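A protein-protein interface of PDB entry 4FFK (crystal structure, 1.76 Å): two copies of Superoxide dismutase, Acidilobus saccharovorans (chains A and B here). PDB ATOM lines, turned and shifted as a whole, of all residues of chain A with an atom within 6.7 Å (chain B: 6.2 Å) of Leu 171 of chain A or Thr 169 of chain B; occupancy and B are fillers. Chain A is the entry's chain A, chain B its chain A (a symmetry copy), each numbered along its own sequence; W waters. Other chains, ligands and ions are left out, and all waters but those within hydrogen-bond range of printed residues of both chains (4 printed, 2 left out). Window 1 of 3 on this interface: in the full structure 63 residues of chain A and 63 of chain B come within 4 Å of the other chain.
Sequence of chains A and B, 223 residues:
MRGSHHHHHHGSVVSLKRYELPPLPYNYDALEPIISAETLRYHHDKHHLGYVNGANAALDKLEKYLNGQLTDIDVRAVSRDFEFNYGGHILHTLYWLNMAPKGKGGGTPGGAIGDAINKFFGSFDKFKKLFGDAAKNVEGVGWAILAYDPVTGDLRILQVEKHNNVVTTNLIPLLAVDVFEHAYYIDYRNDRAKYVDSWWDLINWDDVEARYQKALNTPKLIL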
ATOM      1  N   GLU A  83      -5.233  27.317  -8.737  1.00  0.00           N
ATOM      2  CA  GLU A  83      -4.388  26.915  -9.862  1.00  0.00           C
ATOM      3  C   GLU A  83      -4.182  28.117 -10.778  1.00  0.00           C
ATOM      4  O   GLU A  83      -3.032  28.314 -11.324  1.00  0.00           O
ATOM      5  CB  GLU A  83      -5.041  25.755 -10.593  1.00  0.00           C
ATOM      6  CG  GLU A  83      -4.883  24.536  -9.686  1.00  0.00           C
ATOM      7  CD  GLU A  83      -5.643  23.398 -10.202  1.00  0.00           C
ATOM      8  OE1 GLU A  83      -5.290  22.902 -11.313  1.00  0.00           O
ATOM      9  OE2 GLU A  83      -6.488  22.893  -9.455  1.00  0.00           O
ATOM     10  N   TYR A  86      -1.865  30.491  -8.615  1.00  0.00           N
ATOM     11  CA  TYR A  86      -0.572  29.973  -8.483  1.00  0.00           C
ATOM     12  C   TYR A  86       0.127  30.022  -9.846  1.00  0.00           C
ATOM     13  O   TYR A  86       1.311  30.338  -9.901  1.00  0.00           O
ATOM     14  CB  TYR A  86      -0.609  28.530  -8.061  1.00  0.00           C
ATOM     15  CG  TYR A  86       0.740  27.810  -7.980  1.00  0.00           C
ATOM     16  CD1 TYR A  86       1.254  27.115  -9.082  1.00  0.00           C
ATOM     17  CD2 TYR A  86       1.478  27.795  -6.776  1.00  0.00           C
ATOM     18  CE1 TYR A  86       2.483  26.432  -9.008  1.00  0.00           C
ATOM     19  CE2 TYR A  86       2.639  27.112  -6.690  1.00  0.00           C
ATOM     20  CZ  TYR A  86       3.154  26.467  -7.782  1.00  0.00           C
ATOM     21  OH  TYR A  86       4.301  25.778  -7.647  1.00  0.00           O
ATOM     22  N   GLY A  87      -0.606  29.671 -10.918  1.00  0.00           N
ATOM     23  CA  GLY A  87       0.016  29.760 -12.258  1.00  0.00           C
ATOM     24  C   GLY A  87       0.522  31.192 -12.453  1.00  0.00           C
ATOM     25  O   GLY A  87       1.638  31.398 -12.916  1.00  0.00           O
ATOM     26  N   ILE A  90       3.761  31.802 -10.351  1.00  0.00           N
ATOM     27  CA  ILE A  90       4.937  31.127 -10.744  1.00  0.00           C
ATOM     28  C   ILE A  90       5.399  31.609 -12.093  1.00  0.00           C
ATOM     29  O   ILE A  90       6.589  31.757 -12.333  1.00  0.00           O
ATOM     30  CB  ILE A  90       4.810  29.597 -10.755  1.00  0.00           C
ATOM     31  CG1 ILE A  90       3.815  29.146 -11.853  1.00  0.00           C
ATOM     32  CG2 ILE A  90       4.615  29.063  -9.352  1.00  0.00           C
ATOM     33  CD1 ILE A  90       3.439  27.693 -11.734  1.00  0.00           C
ATOM     34  N   LEU A  91       4.455  31.888 -12.979  1.00  0.00           N
ATOM     35  CA  LEU A  91       4.840  32.333 -14.303  1.00  0.00           C
ATOM     36  C   LEU A  91       5.377  33.751 -14.266  1.00  0.00           C
ATOM     37  O   LEU A  91       6.303  34.085 -15.024  1.00  0.00           O
ATOM     38  CB  LEU A  91       3.673  32.210 -15.284  1.00  0.00           C
ATOM     39  CG  LEU A  91       3.376  30.732 -15.547  1.00  0.00           C
ATOM     40  CD1 LEU A  91       2.084  30.735 -16.421  1.00  0.00           C
ATOM     41  CD2 LEU A  91       4.564  30.081 -16.276  1.00  0.00           C
ATOM     42  N   LEU A  94       8.938  33.538 -12.932  1.00  0.00           N
ATOM     43  CA  LEU A  94       9.800  33.137 -14.055  1.00  0.00           C
ATOM     44  C   LEU A  94      10.039  34.297 -14.988  1.00  0.00           C
ATOM     45  O   LEU A  94      11.206  34.650 -15.327  1.00  0.00           O
ATOM     46  CB  LEU A  94       9.135  31.997 -14.822  1.00  0.00           C
ATOM     47  CG  LEU A  94       9.887  31.417 -16.007  1.00  0.00           C
ATOM     48  CD1 LEU A  94      11.270  30.957 -15.547  1.00  0.00           C
ATOM     49  CD2 LEU A  94       9.087  30.233 -16.558  1.00  0.00           C
ATOM     50  N   ILE A 145       6.017  29.726 -23.595  1.00  0.00           N
ATOM     51  CA  ILE A 145       6.972  29.173 -22.713  1.00  0.00           C
ATOM     52  C   ILE A 145       7.914  28.243 -23.480  1.00  0.00           C
ATOM     53  O   ILE A 145       7.457  27.484 -24.287  1.00  0.00           O
ATOM     54  CB  ILE A 145       6.306  28.350 -21.610  1.00  0.00           C
ATOM     55  CG1 ILE A 145       5.596  29.251 -20.600  1.00  0.00           C
ATOM     56  CG2 ILE A 145       7.379  27.549 -20.895  1.00  0.00           C
ATOM     57  CD1 ILE A 145       4.753  28.437 -19.612  1.00  0.00           C
ATOM     58  N   ALA A 147      10.023  25.207 -22.752  1.00  0.00           N
ATOM     59  CA  ALA A 147      10.078  24.264 -21.669  1.00  0.00           C
ATOM     60  C   ALA A 147      10.992  23.100 -22.001  1.00  0.00           C
ATOM     61  O   ALA A 147      11.236  22.768 -23.171  1.00  0.00           O
ATOM     62  CB  ALA A 147       8.689  23.733 -21.370  1.00  0.00           C
ATOM     63  N   TYR A 148      11.440  22.483 -20.936  1.00  0.00           N
ATOM     64  CA  TYR A 148      12.199  21.247 -21.019  1.00  0.00           C
ATOM     65  C   TYR A 148      11.230  20.088 -20.763  1.00  0.00           C
ATOM     66  O   TYR A 148      10.518  20.121 -19.749  1.00  0.00           O
ATOM     67  CB  TYR A 148      13.274  21.281 -19.941  1.00  0.00           C
ATOM     68  CG  TYR A 148      14.019  19.946 -19.854  1.00  0.00           C
ATOM     69  CD1 TYR A 148      14.861  19.537 -20.895  1.00  0.00           C
ATOM     70  CD2 TYR A 148      13.872  19.103 -18.726  1.00  0.00           C
ATOM     71  CE1 TYR A 148      15.539  18.312 -20.828  1.00  0.00           C
ATOM     72  CE2 TYR A 148      14.553  17.888 -18.650  1.00  0.00           C
ATOM     73  CZ  TYR A 148      15.387  17.514 -19.704  1.00  0.00           C
ATOM     74  OH  TYR A 148      16.063  16.306 -19.666  1.00  0.00           O
ATOM     75  N   ASP A 149      11.210  19.097 -21.649  1.00  0.00           N
ATOM     76  CA  ASP A 149      10.380  17.920 -21.459  1.00  0.00           C
ATOM     77  C   ASP A 149      11.210  16.795 -20.805  1.00  0.00           C
ATOM     78  O   ASP A 149      12.006  16.186 -21.481  1.00  0.00           O
ATOM     79  CB  ASP A 149       9.865  17.410 -22.780  1.00  0.00           C
ATOM     80  CG  ASP A 149       9.167  16.081 -22.641  1.00  0.00           C
ATOM     81  OD1 ASP A 149       8.766  15.740 -21.473  1.00  0.00           O
ATOM     82  OD2 ASP A 149       8.974  15.435 -23.679  1.00  0.00           O
ATOM     83  N   PRO A 150      11.037  16.561 -19.504  1.00  0.00           N
ATOM     84  CA  PRO A 150      11.839  15.500 -18.834  1.00  0.00           C
ATOM     85  C   PRO A 150      11.686  14.125 -19.454  1.00  0.00           C
ATOM     86  O   PRO A 150      12.581  13.268 -19.276  1.00  0.00           O
ATOM     87  CB  PRO A 150      11.311  15.490 -17.401  1.00  0.00           C
ATOM     88  CG  PRO A 150      10.522  16.756 -17.271  1.00  0.00           C
ATOM     89  CD  PRO A 150       9.996  17.083 -18.612  1.00  0.00           C
ATOM     90  N   ASP A 154      13.707  16.719 -24.819  1.00  0.00           N
ATOM     91  CA  ASP A 154      13.453  17.742 -25.868  1.00  0.00           C
ATOM     92  C   ASP A 154      13.021  19.071 -25.226  1.00  0.00           C
ATOM     93  O   ASP A 154      12.383  19.081 -24.175  1.00  0.00           O
ATOM     94  CB  ASP A 154      12.367  17.295 -26.855  1.00  0.00           C
ATOM     95  CG  ASP A 154      12.869  16.328 -27.949  1.00  0.00           C
ATOM     96  OD1 ASP A 154      13.968  15.749 -27.797  1.00  0.00           O
ATOM     97  OD2 ASP A 154      12.197  16.154 -28.980  1.00  0.00           O
ATOM     98  N   ARG A 156      10.441  22.065 -25.686  1.00  0.00           N
ATOM     99  CA  ARG A 156       9.139  22.178 -26.339  1.00  0.00           C
ATOM    100  C   ARG A 156       8.693  23.609 -26.135  1.00  0.00           C
ATOM    101  O   ARG A 156       8.945  24.179 -25.083  1.00  0.00           O
ATOM    102  CB  ARG A 156       8.061  21.289 -25.654  1.00  0.00           C
ATOM    103  CG  ARG A 156       8.303  19.806 -25.740  1.00  0.00           C
ATOM    104  CD  ARG A 156       8.111  19.242 -27.148  1.00  0.00           C
ATOM    105  NE  ARG A 156       8.312  17.784 -27.083  1.00  0.00           N
ATOM    106  CZ  ARG A 156       9.202  17.099 -27.790  1.00  0.00           C
ATOM    107  NH1 ARG A 156       9.936  17.678 -28.738  1.00  0.00           N
ATOM    108  NH2 ARG A 156       9.291  15.794 -27.605  1.00  0.00           N
ATOM    109  N   LEU A 158       5.575  25.881 -25.524  1.00  0.00           N
ATOM    110  CA  LEU A 158       4.184  25.787 -25.083  1.00  0.00           C
ATOM    111  C   LEU A 158       3.483  27.120 -25.240  1.00  0.00           C
ATOM    112  O   LEU A 158       4.084  28.173 -25.094  1.00  0.00           O
ATOM    113  CB  LEU A 158       4.162  25.466 -23.596  1.00  0.00           C
ATOM    114  CG  LEU A 158       5.125  24.305 -23.259  1.00  0.00           C
ATOM    115  CD1 LEU A 158       4.976  24.112 -21.778  1.00  0.00           C
ATOM    116  CD2 LEU A 158       4.859  23.078 -24.020  1.00  0.00           C
ATOM    117  N   VAL A 160       0.319  29.070 -23.114  1.00  0.00           N
ATOM    118  CA  VAL A 160      -0.534  28.973 -21.954  1.00  0.00           C
ATOM    119  C   VAL A 160      -1.618  29.989 -22.200  1.00  0.00           C
ATOM    120  O   VAL A 160      -1.352  31.060 -22.734  1.00  0.00           O
ATOM    121  CB  VAL A 160       0.211  29.416 -20.647  1.00  0.00           C
ATOM    122  CG1 VAL A 160      -0.775  29.181 -19.486  1.00  0.00           C
ATOM    123  CG2 VAL A 160       1.479  28.605 -20.455  1.00  0.00           C
ATOM    124  N   HIS A 163      -3.256  31.654 -16.964  1.00  0.00           N
ATOM    125  CA  HIS A 163      -2.030  31.091 -16.447  1.00  0.00           C
ATOM    126  C   HIS A 163      -2.155  29.621 -16.333  1.00  0.00           C
ATOM    127  O   HIS A 163      -1.252  28.979 -15.799  1.00  0.00           O
ATOM    128  CB  HIS A 163      -1.804  31.603 -15.020  1.00  0.00           C
ATOM    129  CG  HIS A 163      -1.871  33.090 -14.914  1.00  0.00           C
ATOM    130  ND1 HIS A 163      -1.160  33.924 -15.767  1.00  0.00           N
ATOM    131  CD2 HIS A 163      -2.566  33.903 -14.073  1.00  0.00           C
ATOM    132  CE1 HIS A 163      -1.399  35.186 -15.437  1.00  0.00           C
ATOM    133  NE2 HIS A 163      -2.271  35.197 -14.425  1.00  0.00           N
ATOM    134  N   ASN A 164      -3.314  29.077 -16.776  1.00  0.00           N
ATOM    135  CA  ASN A 164      -3.590  27.709 -16.409  1.00  0.00           C
ATOM    136  C   ASN A 164      -4.586  27.063 -17.315  1.00  0.00           C
ATOM    137  O   ASN A 164      -5.416  26.306 -16.840  1.00  0.00           O
ATOM    138  CB  ASN A 164      -4.100  27.670 -14.954  1.00  0.00           C
ATOM    139  CG  ASN A 164      -5.437  28.388 -14.771  1.00  0.00           C
ATOM    140  OD1 ASN A 164      -5.753  29.359 -15.458  1.00  0.00           O
ATOM    141  ND2 ASN A 164      -6.282  27.822 -13.884  1.00  0.00           N
ATOM    142  N   VAL A 167      -1.718  24.689 -21.008  1.00  0.00           N
ATOM    143  CA  VAL A 167      -0.498  24.103 -20.408  1.00  0.00           C
ATOM    144  C   VAL A 167      -0.825  22.841 -19.639  1.00  0.00           C
ATOM    145  O   VAL A 167      -1.972  22.570 -19.281  1.00  0.00           O
ATOM    146  CB  VAL A 167       0.194  25.166 -19.499  1.00  0.00           C
ATOM    147  CG1 VAL A 167      -0.623  25.438 -18.207  1.00  0.00           C
ATOM    148  CG2 VAL A 167       1.716  24.858 -19.251  1.00  0.00           C
ATOM    149  N   THR A 168       0.196  22.014 -19.463  1.00  0.00           N
ATOM    150  CA  THR A 168      -0.011  20.825 -18.680  1.00  0.00           C
ATOM    151  C   THR A 168       1.222  20.691 -17.824  1.00  0.00           C
ATOM    152  O   THR A 168       2.174  21.495 -17.907  1.00  0.00           O
ATOM    153  CB  THR A 168      -0.398  19.597 -19.567  1.00  0.00           C
ATOM    154  OG1 THR A 168      -0.829  18.514 -18.712  1.00  0.00           O
ATOM    155  CG2 THR A 168       0.814  19.120 -20.461  1.00  0.00           C
ATOM    156  N   THR A 169       1.215  19.630 -17.033  1.00  0.00           N
ATOM    157  CA  THR A 169       2.184  19.378 -16.047  1.00  0.00           C
ATOM    158  C   THR A 169       3.470  18.706 -16.631  1.00  0.00           C
ATOM    159  O   THR A 169       3.560  18.461 -17.812  1.00  0.00           O
ATOM    160  CB  THR A 169       1.494  18.498 -14.948  1.00  0.00           C
ATOM    161  OG1 THR A 169       2.307  18.445 -13.792  1.00  0.00           O
ATOM    162  CG2 THR A 169       1.197  17.141 -15.416  1.00  0.00           C
ATOM    163  N   ASN A 170       4.447  18.521 -15.757  1.00  0.00           N
ATOM    164  CA  ASN A 170       5.672  17.753 -16.014  1.00  0.00           C
ATOM    165  C   ASN A 170       6.709  18.514 -16.846  1.00  0.00           C
ATOM    166  O   ASN A 170       7.909  18.538 -16.524  1.00  0.00           O
ATOM    167  CB  ASN A 170       5.389  16.411 -16.645  1.00  0.00           C
ATOM    168  CG  ASN A 170       6.534  15.408 -16.346  1.00  0.00           C
ATOM    169  OD1 ASN A 170       6.999  15.337 -15.211  1.00  0.00           O
ATOM    170  ND2 ASN A 170       7.023  14.722 -17.363  1.00  0.00           N
ATOM    171  N   LEU A 171       6.250  19.122 -17.922  1.00  0.00           N
ATOM    172  CA  LEU A 171       7.081  20.107 -18.651  1.00  0.00           C
ATOM    173  C   LEU A 171       7.635  21.133 -17.706  1.00  0.00           C
ATOM    174  O   LEU A 171       6.932  21.660 -16.832  1.00  0.00           O
ATOM    175  CB  LEU A 171       6.233  20.789 -19.729  1.00  0.00           C
ATOM    176  CG  LEU A 171       5.759  19.777 -20.736  1.00  0.00           C
ATOM    177  CD1 LEU A 171       4.459  20.232 -21.415  1.00  0.00           C
ATOM    178  CD2 LEU A 171       6.913  19.492 -21.705  1.00  0.00           C
ATOM    179  N   ILE A 172       8.922  21.458 -17.876  1.00  0.00           N
ATOM    180  CA  ILE A 172       9.599  22.389 -17.014  1.00  0.00           C
ATOM    181  C   ILE A 172       9.840  23.682 -17.795  1.00  0.00           C
ATOM    182  O   ILE A 172      10.568  23.686 -18.784  1.00  0.00           O
ATOM    183  CB  ILE A 172      10.968  21.801 -16.552  1.00  0.00           C
ATOM    184  CG1 ILE A 172      10.725  20.407 -15.906  1.00  0.00           C
ATOM    185  CG2 ILE A 172      11.805  22.822 -15.727  1.00  0.00           C
ATOM    186  CD1 ILE A 172      11.967  19.759 -15.303  1.00  0.00           C
ATOM    187  N   PRO A 173       9.189  24.761 -17.369  1.00  0.00           N
ATOM    188  CA  PRO A 173       9.299  26.012 -18.134  1.00  0.00           C
ATOM    189  C   PRO A 173      10.692  26.556 -17.862  1.00  0.00           C
ATOM    190  O   PRO A 173      11.116  26.566 -16.723  1.00  0.00           O
ATOM    191  CB  PRO A 173       8.256  26.922 -17.484  1.00  0.00           C
ATOM    192  CG  PRO A 173       8.119  26.330 -16.021  1.00  0.00           C
ATOM    193  CD  PRO A 173       8.183  24.811 -16.294  1.00  0.00           C
ATOM    194  N   TYR B  19       6.953  10.129 -28.478  1.00  0.00           N
ATOM    195  CA  TYR B  19       6.471   9.478 -27.258  1.00  0.00           C
ATOM    196  C   TYR B  19       6.121   8.031 -27.452  1.00  0.00           C
ATOM    197  O   TYR B  19       5.721   7.617 -28.511  1.00  0.00           O
ATOM    198  CB  TYR B  19       5.283  10.254 -26.635  1.00  0.00           C
ATOM    199  CG  TYR B  19       5.738  11.635 -26.281  1.00  0.00           C
ATOM    200  CD1 TYR B  19       6.431  11.882 -25.118  1.00  0.00           C
ATOM    201  CD2 TYR B  19       5.524  12.702 -27.169  1.00  0.00           C
ATOM    202  CE1 TYR B  19       6.919  13.117 -24.834  1.00  0.00           C
ATOM    203  CE2 TYR B  19       6.044  13.936 -26.892  1.00  0.00           C
ATOM    204  CZ  TYR B  19       6.713  14.147 -25.721  1.00  0.00           C
ATOM    205  OH  TYR B  19       7.203  15.384 -25.389  1.00  0.00           O
ATOM    206  N   PHE B  82      -0.178  19.581 -28.998  1.00  0.00           N
ATOM    207  CA  PHE B  82       0.895  18.954 -28.298  1.00  0.00           C
ATOM    208  C   PHE B  82       0.561  18.868 -26.790  1.00  0.00           C
ATOM    209  O   PHE B  82       0.735  17.832 -26.149  1.00  0.00           O
ATOM    210  CB  PHE B  82       2.216  19.712 -28.454  1.00  0.00           C
ATOM    211  CG  PHE B  82       3.252  19.250 -27.506  1.00  0.00           C
ATOM    212  CD1 PHE B  82       3.664  20.032 -26.425  1.00  0.00           C
ATOM    213  CD2 PHE B  82       3.751  17.918 -27.632  1.00  0.00           C
ATOM    214  CE1 PHE B  82       4.619  19.499 -25.509  1.00  0.00           C
ATOM    215  CE2 PHE B  82       4.653  17.448 -26.740  1.00  0.00           C
ATOM    216  CZ  PHE B  82       5.063  18.205 -25.679  1.00  0.00           C
ATOM    217  N   GLU B  83       0.093  19.982 -26.262  1.00  0.00           N
ATOM    218  CA  GLU B  83      -0.029  20.132 -24.811  1.00  0.00           C
ATOM    219  C   GLU B  83      -1.179  19.259 -24.320  1.00  0.00           C
ATOM    220  O   GLU B  83      -1.067  18.622 -23.206  1.00  0.00           O
ATOM    221  CB  GLU B  83      -0.248  21.596 -24.473  1.00  0.00           C
ATOM    222  CG  GLU B  83       1.091  22.293 -24.706  1.00  0.00           C
ATOM    223  CD  GLU B  83       0.951  23.745 -24.595  1.00  0.00           C
ATOM    224  OE1 GLU B  83       0.638  24.227 -23.466  1.00  0.00           O
ATOM    225  OE2 GLU B  83       1.294  24.424 -25.568  1.00  0.00           O
ATOM    226  N   TYR B  86       0.224  15.588 -24.810  1.00  0.00           N
ATOM    227  CA  TYR B  86       1.247  15.299 -23.901  1.00  0.00           C
ATOM    228  C   TYR B  86       0.652  15.213 -22.490  1.00  0.00           C
ATOM    229  O   TYR B  86       1.053  14.345 -21.722  1.00  0.00           O
ATOM    230  CB  TYR B  86       2.274  16.397 -23.876  1.00  0.00           C
ATOM    231  CG  TYR B  86       3.398  16.255 -22.845  1.00  0.00           C
ATOM    232  CD1 TYR B  86       3.278  16.813 -21.566  1.00  0.00           C
ATOM    233  CD2 TYR B  86       4.601  15.593 -23.177  1.00  0.00           C
ATOM    234  CE1 TYR B  86       4.315  16.705 -20.621  1.00  0.00           C
ATOM    235  CE2 TYR B  86       5.612  15.518 -22.286  1.00  0.00           C
ATOM    236  CZ  TYR B  86       5.473  16.033 -21.024  1.00  0.00           C
ATOM    237  OH  TYR B  86       6.513  15.959 -20.176  1.00  0.00           O
ATOM    238  N   ILE B  90       1.227  11.966 -20.092  1.00  0.00           N
ATOM    239  CA  ILE B  90       1.917  11.991 -18.860  1.00  0.00           C
ATOM    240  C   ILE B  90       0.982  11.673 -17.724  1.00  0.00           C
ATOM    241  O   ILE B  90       1.348  10.983 -16.784  1.00  0.00           O
ATOM    242  CB  ILE B  90       2.650  13.309 -18.576  1.00  0.00           C
ATOM    243  CG1 ILE B  90       1.633  14.462 -18.383  1.00  0.00           C
ATOM    244  CG2 ILE B  90       3.785  13.516 -19.557  1.00  0.00           C
ATOM    245  CD1 ILE B  90       2.287  15.818 -18.377  1.00  0.00           C
ATOM    246  N   VAL B 167      -5.066  23.183 -14.730  1.00  0.00           N
ATOM    247  CA  VAL B 167      -3.726  22.877 -14.179  1.00  0.00           C
ATOM    248  C   VAL B 167      -2.707  23.897 -14.636  1.00  0.00           C
ATOM    249  O   VAL B 167      -2.907  24.638 -15.601  1.00  0.00           O
ATOM    250  CB  VAL B 167      -3.316  21.429 -14.592  1.00  0.00           C
ATOM    251  CG1 VAL B 167      -2.998  21.332 -16.108  1.00  0.00           C
ATOM    252  CG2 VAL B 167      -2.208  20.821 -13.657  1.00  0.00           C
ATOM    253  N   THR B 168      -1.630  23.994 -13.869  1.00  0.00           N
ATOM    254  CA  THR B 168      -0.578  24.888 -14.271  1.00  0.00           C
ATOM    255  C   THR B 168       0.704  24.144 -13.997  1.00  0.00           C
ATOM    256  O   THR B 168       0.711  23.006 -13.482  1.00  0.00           O
ATOM    257  CB  THR B 168      -0.731  26.304 -13.628  1.00  0.00           C
ATOM    258  OG1 THR B 168       0.200  27.213 -14.258  1.00  0.00           O
ATOM    259  CG2 THR B 168      -0.469  26.266 -12.070  1.00  0.00           C
ATOM    260  N   THR B 169       1.797  24.827 -14.299  1.00  0.00           N
ATOM    261  CA  THR B 169       3.095  24.289 -14.266  1.00  0.00           C
ATOM    262  C   THR B 169       3.709  24.299 -12.827  1.00  0.00           C
ATOM    263  O   THR B 169       3.082  24.731 -11.888  1.00  0.00           O
ATOM    264  CB  THR B 169       3.952  25.111 -15.289  1.00  0.00           C
ATOM    265  OG1 THR B 169       5.181  24.451 -15.527  1.00  0.00           O
ATOM    266  CG2 THR B 169       4.197  26.486 -14.844  1.00  0.00           C
ATOM    267  N   ASN B 170       4.899  23.728 -12.726  1.00  0.00           N
ATOM    268  CA  ASN B 170       5.754  23.771 -11.534  1.00  0.00           C
ATOM    269  C   ASN B 170       5.318  22.800 -10.431  1.00  0.00           C
ATOM    270  O   ASN B 170       6.137  22.073  -9.845  1.00  0.00           O
ATOM    271  CB  ASN B 170       5.888  25.165 -10.970  1.00  0.00           C
ATOM    272  CG  ASN B 170       7.205  25.309 -10.161  1.00  0.00           C
ATOM    273  OD1 ASN B 170       8.251  24.854 -10.616  1.00  0.00           O
ATOM    274  ND2 ASN B 170       7.125  25.854  -8.961  1.00  0.00           N
ATOM    275  N   LEU B 171       4.032  22.801 -10.140  1.00  0.00           N
ATOM    276  CA  LEU B 171       3.443  21.732  -9.302  1.00  0.00           C
ATOM    277  C   LEU B 171       3.827  20.378  -9.825  1.00  0.00           C
ATOM    278  O   LEU B 171       3.785  20.111 -11.035  1.00  0.00           O
ATOM    279  CB  LEU B 171       1.918  21.877  -9.291  1.00  0.00           C
ATOM    280  CG  LEU B 171       1.524  23.191  -8.675  1.00  0.00           C
ATOM    281  CD1 LEU B 171       0.160  23.665  -9.194  1.00  0.00           C
ATOM    282  CD2 LEU B 171       1.606  23.045  -7.150  1.00  0.00           C
ATOM    283  N   ILE B 172       4.198  19.475  -8.910  1.00  0.00           N
ATOM    284  CA  ILE B 172       4.639  18.155  -9.269  1.00  0.00           C
ATOM    285  C   ILE B 172       3.550  17.157  -8.869  1.00  0.00           C
ATOM    286  O   ILE B 172       3.248  17.005  -7.689  1.00  0.00           O
ATOM    287  CB  ILE B 172       5.962  17.804  -8.519  1.00  0.00           C
ATOM    288  CG1 ILE B 172       7.011  18.917  -8.804  1.00  0.00           C
ATOM    289  CG2 ILE B 172       6.412  16.334  -8.767  1.00  0.00           C
ATOM    290  CD1 ILE B 172       8.397  18.649  -8.225  1.00  0.00           C
ATOM    291  N   ILE B 222      12.119  27.525 -10.083  1.00  0.00           N
ATOM    292  CA  ILE B 222      11.712  28.884 -10.293  1.00  0.00           C
ATOM    293  C   ILE B 222      11.839  29.678  -9.028  1.00  0.00           C
ATOM    294  O   ILE B 222      12.424  30.745  -9.039  1.00  0.00           O
ATOM    295  CB  ILE B 222      10.260  28.974 -10.851  1.00  0.00           C
ATOM    296  CG1 ILE B 222      10.157  28.235 -12.209  1.00  0.00           C
ATOM    297  CG2 ILE B 222       9.845  30.424 -10.952  1.00  0.00           C
ATOM    298  CD1 ILE B 222       8.709  28.066 -12.758  1.00  0.00           C
HETATM  299  O   HOH W   1       4.363  22.189 -16.656  1.00  0.00           O
HETATM  300  O   HOH W   2       6.468  21.893 -14.294  1.00  0.00           O
HETATM  301  O   HOH W   3       2.314  20.990 -13.028  1.00  0.00           O
HETATM  302  O   HOH W   4       5.149  19.564 -13.168  1.00  0.00           O
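The side-chain carboxylate of Asp 149 of chain A lies within hydrogen-bond range of the side-chain hydroxyl of Tyr 86 of chain B, at 2.6 Å.
The side-chain carboxylate (OE1) of Glu 83 of chain A sits close to the backbone NH (N) of Val 167 of chain B, 3.4 Å away.
The backbone carbonyl oxygen (O) of His 163 of chain A is in hydrogen-bond range of the side-chain hydroxyl (OG1) of Thr 168 of chain B (2.8 Å).
ND2 of Asn 170 of chain B lies within hydrogen-bond range of OH of Tyr 86 of chain A, at 3.1 Å.
OH of Tyr 19 of chain B is in hydrogen-bond range of OD2 of Asp 149 of chain A.
The side-chain hydroxyl (OH) of Tyr 86 of chain B sits at hydrogen-bond distance from the side-chain amide nitrogen (ND2) of Asn 170 of chain A.
The side-chain carboxylate (OE1) of Glu 83 of chain B sits close to the backbone NH (N) of Val 167 of chain A, 3.4 Å away.
The guanidinium group (NH2) of Arg 156 of chain A is in hydrogen-bond range of the side-chain hydroxyl (OH) of Tyr 19 of chain B.
O of Val 167 of chain B sits close to O of Asn 164 of chain A (3.3 Å).
The side-chain carboxylate (OD2) of Asp 149 of chain A is in salt-bridge range of the guanidinium group (NH2) of Arg 156 of chain A.
Leu 171 of chain A touches just these residues of chain B: Tyr 86 and Thr 169.
Thr 169 of chain B touches just these residues of chain A: Tyr 86, Ile 90, Leu 91, Leu 171 and Pro 173.
Printed residues of chain B within 4 Å of Gly 87 of chain A: Thr 168.
Of the printed residues of chain B, Leu 158 of chain A touches Phe 82 (3.9 Å) and Glu 83 (3.2 Å).
Ile 172 of chain B touches none of the printed residues of chain A.
The nearest residue of chain B that does not touch Leu 171 of chain A is Phe 82 of chain B (4.2 Å).
The nearest printed residue of chain B that does not touch Asn 164 of chain A is Thr 169 of chain B (6.5 Å).
Of the 12 printed residues of chain B, 11 touch a printed residue of chain A.
Hydrophobic or aromatic side chains of chain A that line the printed part of chain B: Tyr 86, Ile 90, Leu 91, Pro 150, Leu 158, Val 167, Leu 171 and Pro 173.
Among the printed residues, 37 pairs touch across the chains.
Among the printed residues, no Asp or Glu carboxylate lies within 4 Å of a Lys or Arg side-chain nitrogen of the other chain.
Tyr 86 of chain A touches Asn 170 of chain B, and with the chains exchanged Asn 170 of chain A touches Tyr 86 of chain B.
Val 167 of chain A touches its own counterpart, Val 167 of chain B.
Water W3 lies within hydrogen-bond range of the backbone carbonyl oxygen of Thr 168 of chain B (2.6 Å), the backbone carbonyl oxygen of Leu 171 of chain B (2.6 Å) and the side-chain hydroxyl of Thr 169 of chain A (2.7 Å).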
